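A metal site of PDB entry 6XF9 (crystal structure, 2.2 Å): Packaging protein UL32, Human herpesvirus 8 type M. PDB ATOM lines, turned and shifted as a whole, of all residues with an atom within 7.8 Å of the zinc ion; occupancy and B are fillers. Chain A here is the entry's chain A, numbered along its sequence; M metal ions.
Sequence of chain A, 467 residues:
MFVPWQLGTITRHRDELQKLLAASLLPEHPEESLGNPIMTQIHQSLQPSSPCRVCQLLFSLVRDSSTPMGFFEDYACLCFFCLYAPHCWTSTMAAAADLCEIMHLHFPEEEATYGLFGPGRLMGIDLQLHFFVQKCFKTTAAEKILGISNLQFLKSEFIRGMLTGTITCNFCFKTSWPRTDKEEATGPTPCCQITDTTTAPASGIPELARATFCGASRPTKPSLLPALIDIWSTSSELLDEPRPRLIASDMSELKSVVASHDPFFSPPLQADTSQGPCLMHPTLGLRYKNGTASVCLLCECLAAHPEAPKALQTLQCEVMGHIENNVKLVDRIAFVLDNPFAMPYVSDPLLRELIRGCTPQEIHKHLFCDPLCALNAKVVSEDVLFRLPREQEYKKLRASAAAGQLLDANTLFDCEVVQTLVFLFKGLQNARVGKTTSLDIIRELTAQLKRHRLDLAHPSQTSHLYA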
ATOM      1  N   HIS A  87     -19.491 -21.409   6.376  1.00  0.00           N
ATOM      2  CA  HIS A  87     -18.504 -22.324   5.811  1.00  0.00           C
ATOM      3  C   HIS A  87     -19.005 -23.881   5.668  1.00  0.00           C
ATOM      4  O   HIS A  87     -19.399 -24.641   6.596  1.00  0.00           O
ATOM      5  CB  HIS A  87     -17.251 -22.240   6.657  1.00  0.00           C
ATOM      6  CG  HIS A  87     -16.022 -22.651   5.933  1.00  0.00           C
ATOM      7  ND1 HIS A  87     -14.767 -22.222   6.297  1.00  0.00           N
ATOM      8  CD2 HIS A  87     -15.849 -23.435   4.842  1.00  0.00           C
ATOM      9  CE1 HIS A  87     -13.880 -22.738   5.465  1.00  0.00           C
ATOM     10  NE2 HIS A  87     -14.505 -23.469   4.578  1.00  0.00           N
ATOM     11  N   VAL A 295     -19.550 -33.879   8.126  1.00  0.00           N
ATOM     12  CA  VAL A 295     -20.220 -32.917   7.243  1.00  0.00           C
ATOM     13  C   VAL A 295     -21.615 -32.689   7.811  1.00  0.00           C
ATOM     14  O   VAL A 295     -22.468 -33.587   7.795  1.00  0.00           O
ATOM     15  CB  VAL A 295     -20.280 -33.406   5.786  1.00  0.00           C
ATOM     16  CG1 VAL A 295     -21.103 -32.432   4.938  1.00  0.00           C
ATOM     17  CG2 VAL A 295     -18.888 -33.531   5.214  1.00  0.00           C
ATOM     18  N   CYS A 296     -21.874 -31.487   8.313  1.00  0.00           N
ATOM     19  CA  CYS A 296     -23.158 -31.217   8.925  1.00  0.00           C
ATOM     20  C   CYS A 296     -24.155 -30.829   7.845  1.00  0.00           C
ATOM     21  O   CYS A 296     -23.878 -29.949   7.022  1.00  0.00           O
ATOM     22  CB  CYS A 296     -23.045 -30.114   9.948  1.00  0.00           C
ATOM     23  SG  CYS A 296     -24.627 -29.645  10.660  1.00  0.00           S
ATOM     24  N   LEU A 297     -25.284 -31.542   7.815  1.00  0.00           N
ATOM     25  CA  LEU A 297     -26.275 -31.312   6.763  1.00  0.00           C
ATOM     26  C   LEU A 297     -27.106 -30.062   7.018  1.00  0.00           C
ATOM     27  O   LEU A 297     -27.539 -29.412   6.065  1.00  0.00           O
ATOM     28  CB  LEU A 297     -27.185 -32.527   6.642  1.00  0.00           C
ATOM     29  CG  LEU A 297     -27.776 -32.834   5.270  1.00  0.00           C
ATOM     30  CD1 LEU A 297     -26.715 -32.922   4.217  1.00  0.00           C
ATOM     31  CD2 LEU A 297     -28.405 -34.185   5.397  1.00  0.00           C
ATOM     32  N   LEU A 298     -27.353 -29.731   8.281  1.00  0.00           N
ATOM     33  CA  LEU A 298     -28.080 -28.512   8.583  1.00  0.00           C
ATOM     34  C   LEU A 298     -27.230 -27.275   8.313  1.00  0.00           C
ATOM     35  O   LEU A 298     -27.786 -26.221   8.021  1.00  0.00           O
ATOM     36  CB  LEU A 298     -28.565 -28.520  10.024  1.00  0.00           C
ATOM     37  CG  LEU A 298     -29.335 -29.801  10.352  1.00  0.00           C
ATOM     38  CD1 LEU A 298     -29.707 -29.860  11.815  1.00  0.00           C
ATOM     39  CD2 LEU A 298     -30.603 -29.819   9.526  1.00  0.00           C
ATOM     40  N   CYS A 299     -25.903 -27.364   8.403  1.00  0.00           N
ATOM     41  CA  CYS A 299     -25.109 -26.212   7.968  1.00  0.00           C
ATOM     42  C   CYS A 299     -25.165 -26.045   6.474  1.00  0.00           C
ATOM     43  O   CYS A 299     -25.002 -24.939   5.966  1.00  0.00           O
ATOM     44  CB  CYS A 299     -23.643 -26.325   8.379  1.00  0.00           C
ATOM     45  SG  CYS A 299     -23.275 -25.986  10.083  1.00  0.00           S
ATOM     46  N   GLU A 300     -25.277 -27.160   5.743  1.00  0.00           N
ATOM     47  CA  GLU A 300     -25.462 -27.080   4.296  1.00  0.00           C
ATOM     48  C   GLU A 300     -26.747 -26.341   3.948  1.00  0.00           C
ATOM     49  O   GLU A 300     -26.779 -25.550   3.013  1.00  0.00           O
ATOM     50  CB  GLU A 300     -25.448 -28.480   3.692  1.00  0.00           C
ATOM     51  CG  GLU A 300     -24.154 -29.237   3.955  1.00  0.00           C
ATOM     52  CD  GLU A 300     -22.949 -28.515   3.386  1.00  0.00           C
ATOM     53  OE1 GLU A 300     -23.125 -27.887   2.316  1.00  0.00           O
ATOM     54  OE2 GLU A 300     -21.859 -28.548   4.033  1.00  0.00           O
ATOM     55  N   CYS A 301     -27.825 -26.625   4.687  1.00  0.00           N
ATOM     56  CA  CYS A 301     -29.087 -25.946   4.443  1.00  0.00           C
ATOM     57  C   CYS A 301     -28.988 -24.446   4.693  1.00  0.00           C
ATOM     58  O   CYS A 301     -29.689 -23.662   4.041  1.00  0.00           O
ATOM     59  CB  CYS A 301     -30.177 -26.550   5.308  1.00  0.00           C
ATOM     60  SG  CYS A 301     -30.543 -28.255   4.818  1.00  0.00           S
ATOM     61  N   LEU A 302     -28.193 -24.016   5.674  1.00  0.00           N
ATOM     62  CA  LEU A 302     -28.050 -22.585   5.932  1.00  0.00           C
ATOM     63  C   LEU A 302     -27.628 -21.851   4.663  1.00  0.00           C
ATOM     64  O   LEU A 302     -28.070 -20.719   4.414  1.00  0.00           O
ATOM     65  CB  LEU A 302     -27.012 -22.348   7.050  1.00  0.00           C
ATOM     66  CG  LEU A 302     -27.442 -22.859   8.431  1.00  0.00           C
ATOM     67  CD1 LEU A 302     -26.452 -22.517   9.503  1.00  0.00           C
ATOM     68  CD2 LEU A 302     -28.786 -22.311   8.800  1.00  0.00           C
ATOM     69  N   LEU A 312     -34.438 -23.122  11.500  1.00  0.00           N
ATOM     70  CA  LEU A 312     -33.624 -23.765  12.526  1.00  0.00           C
ATOM     71  C   LEU A 312     -33.713 -22.985  13.822  1.00  0.00           C
ATOM     72  O   LEU A 312     -33.862 -23.598  14.892  1.00  0.00           O
ATOM     73  CB  LEU A 312     -32.192 -23.908  12.027  1.00  0.00           C
ATOM     74  CG  LEU A 312     -32.119 -24.930  10.880  1.00  0.00           C
ATOM     75  CD1 LEU A 312     -30.811 -24.893  10.129  1.00  0.00           C
ATOM     76  CD2 LEU A 312     -32.348 -26.321  11.442  1.00  0.00           C
ATOM     77  N   GLU A 362     -27.862 -35.232  15.081  1.00  0.00           N
ATOM     78  CA  GLU A 362     -27.463 -34.189  14.136  1.00  0.00           C
ATOM     79  C   GLU A 362     -28.027 -32.843  14.564  1.00  0.00           C
ATOM     80  O   GLU A 362     -27.361 -31.810  14.438  1.00  0.00           O
ATOM     81  CB  GLU A 362     -27.925 -34.498  12.713  1.00  0.00           C
ATOM     82  CG  GLU A 362     -27.400 -35.801  12.153  1.00  0.00           C
ATOM     83  CD  GLU A 362     -27.588 -35.937  10.650  1.00  0.00           C
ATOM     84  OE1 GLU A 362     -28.471 -36.725  10.245  1.00  0.00           O
ATOM     85  OE2 GLU A 362     -26.870 -35.250   9.884  1.00  0.00           O
ATOM     86  N   ILE A 363     -29.286 -32.837  15.015  1.00  0.00           N
ATOM     87  CA  ILE A 363     -29.955 -31.595  15.389  1.00  0.00           C
ATOM     88  C   ILE A 363     -29.419 -31.070  16.715  1.00  0.00           C
ATOM     89  O   ILE A 363     -29.102 -29.883  16.829  1.00  0.00           O
ATOM     90  CB  ILE A 363     -31.474 -31.824  15.413  1.00  0.00           C
ATOM     91  CG1 ILE A 363     -31.965 -31.970  13.958  1.00  0.00           C
ATOM     92  CG2 ILE A 363     -32.186 -30.721  16.209  1.00  0.00           C
ATOM     93  CD1 ILE A 363     -33.288 -32.643  13.817  1.00  0.00           C
ATOM     94  N   LYS A 365     -26.428 -31.671  17.849  1.00  0.00           N
ATOM     95  CA  LYS A 365     -25.085 -31.191  17.529  1.00  0.00           C
ATOM     96  C   LYS A 365     -25.103 -29.793  16.941  1.00  0.00           C
ATOM     97  O   LYS A 365     -24.307 -28.942  17.340  1.00  0.00           O
ATOM     98  CB  LYS A 365     -24.370 -32.147  16.577  1.00  0.00           C
ATOM     99  CG  LYS A 365     -23.117 -31.565  15.948  1.00  0.00           C
ATOM    100  CD  LYS A 365     -22.492 -32.437  14.862  1.00  0.00           C
ATOM    101  CE  LYS A 365     -21.547 -31.551  14.024  1.00  0.00           C
ATOM    102  NZ  LYS A 365     -20.626 -32.269  13.054  1.00  0.00           N
ATOM    103  N   HIS A 366     -26.020 -29.530  16.002  1.00  0.00           N
ATOM    104  CA  HIS A 366     -26.029 -28.279  15.232  1.00  0.00           C
ATOM    105  C   HIS A 366     -26.594 -27.105  16.035  1.00  0.00           C
ATOM    106  O   HIS A 366     -26.165 -25.955  15.848  1.00  0.00           O
ATOM    107  CB  HIS A 366     -26.843 -28.453  13.934  1.00  0.00           C
ATOM    108  CG  HIS A 366     -27.034 -27.191  13.155  1.00  0.00           C
ATOM    109  ND1 HIS A 366     -26.093 -26.702  12.282  1.00  0.00           N
ATOM    110  CD2 HIS A 366     -28.055 -26.293  13.151  1.00  0.00           C
ATOM    111  CE1 HIS A 366     -26.534 -25.564  11.753  1.00  0.00           C
ATOM    112  NE2 HIS A 366     -27.716 -25.298  12.270  1.00  0.00           N
ATOM    113  N   LEU A 367     -27.606 -27.350  16.867  1.00  0.00           N
ATOM    114  CA  LEU A 367     -28.250 -26.243  17.575  1.00  0.00           C
ATOM    115  C   LEU A 367     -27.608 -25.931  18.921  1.00  0.00           C
ATOM    116  O   LEU A 367     -27.634 -24.777  19.374  1.00  0.00           O
ATOM    117  CB  LEU A 367     -29.733 -26.577  17.790  1.00  0.00           C
ATOM    118  CG  LEU A 367     -30.606 -26.624  16.548  1.00  0.00           C
ATOM    119  CD1 LEU A 367     -31.952 -27.213  16.909  1.00  0.00           C
ATOM    120  CD2 LEU A 367     -30.757 -25.252  15.969  1.00  0.00           C
ATOM    121  N   ASP A 370     -22.074 -27.976  18.581  1.00  0.00           N
ATOM    122  CA  ASP A 370     -20.869 -27.778  17.773  1.00  0.00           C
ATOM    123  C   ASP A 370     -20.528 -26.295  17.642  1.00  0.00           C
ATOM    124  O   ASP A 370     -21.395 -25.491  17.288  1.00  0.00           O
ATOM    125  CB  ASP A 370     -21.025 -28.414  16.397  1.00  0.00           C
ATOM    126  CG  ASP A 370     -19.719 -28.414  15.600  1.00  0.00           C
ATOM    127  OD1 ASP A 370     -19.369 -27.367  15.004  1.00  0.00           O
ATOM    128  OD2 ASP A 370     -19.037 -29.456  15.564  1.00  0.00           O
ATOM    129  N   LEU A 372     -18.589 -24.860  15.331  1.00  0.00           N
ATOM    130  CA  LEU A 372     -18.655 -24.398  13.939  1.00  0.00           C
ATOM    131  C   LEU A 372     -20.100 -24.230  13.495  1.00  0.00           C
ATOM    132  O   LEU A 372     -20.402 -23.312  12.712  1.00  0.00           O
ATOM    133  CB  LEU A 372     -17.894 -25.360  13.011  1.00  0.00           C
ATOM    134  CG  LEU A 372     -17.879 -25.044  11.492  1.00  0.00           C
ATOM    135  CD1 LEU A 372     -17.301 -23.635  11.218  1.00  0.00           C
ATOM    136  CD2 LEU A 372     -17.124 -26.115  10.682  1.00  0.00           C
ATOM    137  N   CYS A 373     -21.011 -25.092  13.957  1.00  0.00           N
ATOM    138  CA  CYS A 373     -22.437 -24.889  13.685  1.00  0.00           C
ATOM    139  C   CYS A 373     -22.929 -23.598  14.298  1.00  0.00           C
ATOM    140  O   CYS A 373     -23.757 -22.889  13.720  1.00  0.00           O
ATOM    141  CB  CYS A 373     -23.281 -26.055  14.219  1.00  0.00           C
ATOM    142  SG  CYS A 373     -22.981 -27.677  13.454  1.00  0.00           S
ATOM    143  N   ALA A 374     -22.461 -23.286  15.508  1.00  0.00           N
ATOM    144  CA  ALA A 374     -22.867 -22.031  16.114  1.00  0.00           C
ATOM    145  C   ALA A 374     -22.359 -20.857  15.295  1.00  0.00           C
ATOM    146  O   ALA A 374     -23.085 -19.918  15.004  1.00  0.00           O
ATOM    147  CB  ALA A 374     -22.360 -21.957  17.562  1.00  0.00           C
ATOM    148  N   ASN A 376     -21.564 -20.770  12.061  1.00  0.00           N
ATOM    149  CA  ASN A 376     -22.244 -20.695  10.765  1.00  0.00           C
ATOM    150  C   ASN A 376     -23.618 -20.048  10.879  1.00  0.00           C
ATOM    151  O   ASN A 376     -24.003 -19.233  10.032  1.00  0.00           O
ATOM    152  CB  ASN A 376     -22.363 -22.094  10.159  1.00  0.00           C
ATOM    153  CG  ASN A 376     -21.115 -22.519   9.428  1.00  0.00           C
ATOM    154  OD1 ASN A 376     -20.199 -21.719   9.193  1.00  0.00           O
ATOM    155  ND2 ASN A 376     -21.086 -23.801   9.038  1.00  0.00           N
ATOM    156  N   ALA A 377     -24.397 -20.435  11.907  1.00  0.00           N
ATOM    157  CA  ALA A 377     -25.704 -19.825  12.136  1.00  0.00           C
ATOM    158  C   ALA A 377     -25.614 -18.330  12.469  1.00  0.00           C
ATOM    159  O   ALA A 377     -26.517 -17.576  12.122  1.00  0.00           O
ATOM    160  CB  ALA A 377     -26.419 -20.558  13.250  1.00  0.00           C
HETATM  161 ZN    ZN M   1     -24.217 -27.539  11.495  1.00  0.00          ZN
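The side-chain sulfur (SG) of Cys 299 lies close to the side-chain amide nitrogen (ND2) of Asn 376.
N of Cys 373 is in hydrogen-bond range of OD1 of Asp 370 (3.0 Å).
SG of Cys 296 lies close to N of Leu 298, at 3.6 Å.
The zinc ion is bound by a ring nitrogen (ND1) of His 366 (2.2 Å), the side-chain sulfur (SG) of Cys 299 (2.3 Å), the side-chain sulfur (SG) of Cys 296 (2.3 Å) and the side-chain sulfur (SG) of Cys 373 (2.3 Å).
Four residues have an atom within 4 Å of the zinc ion: Cys 296, Cys 299, His 366 and Cys 373.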
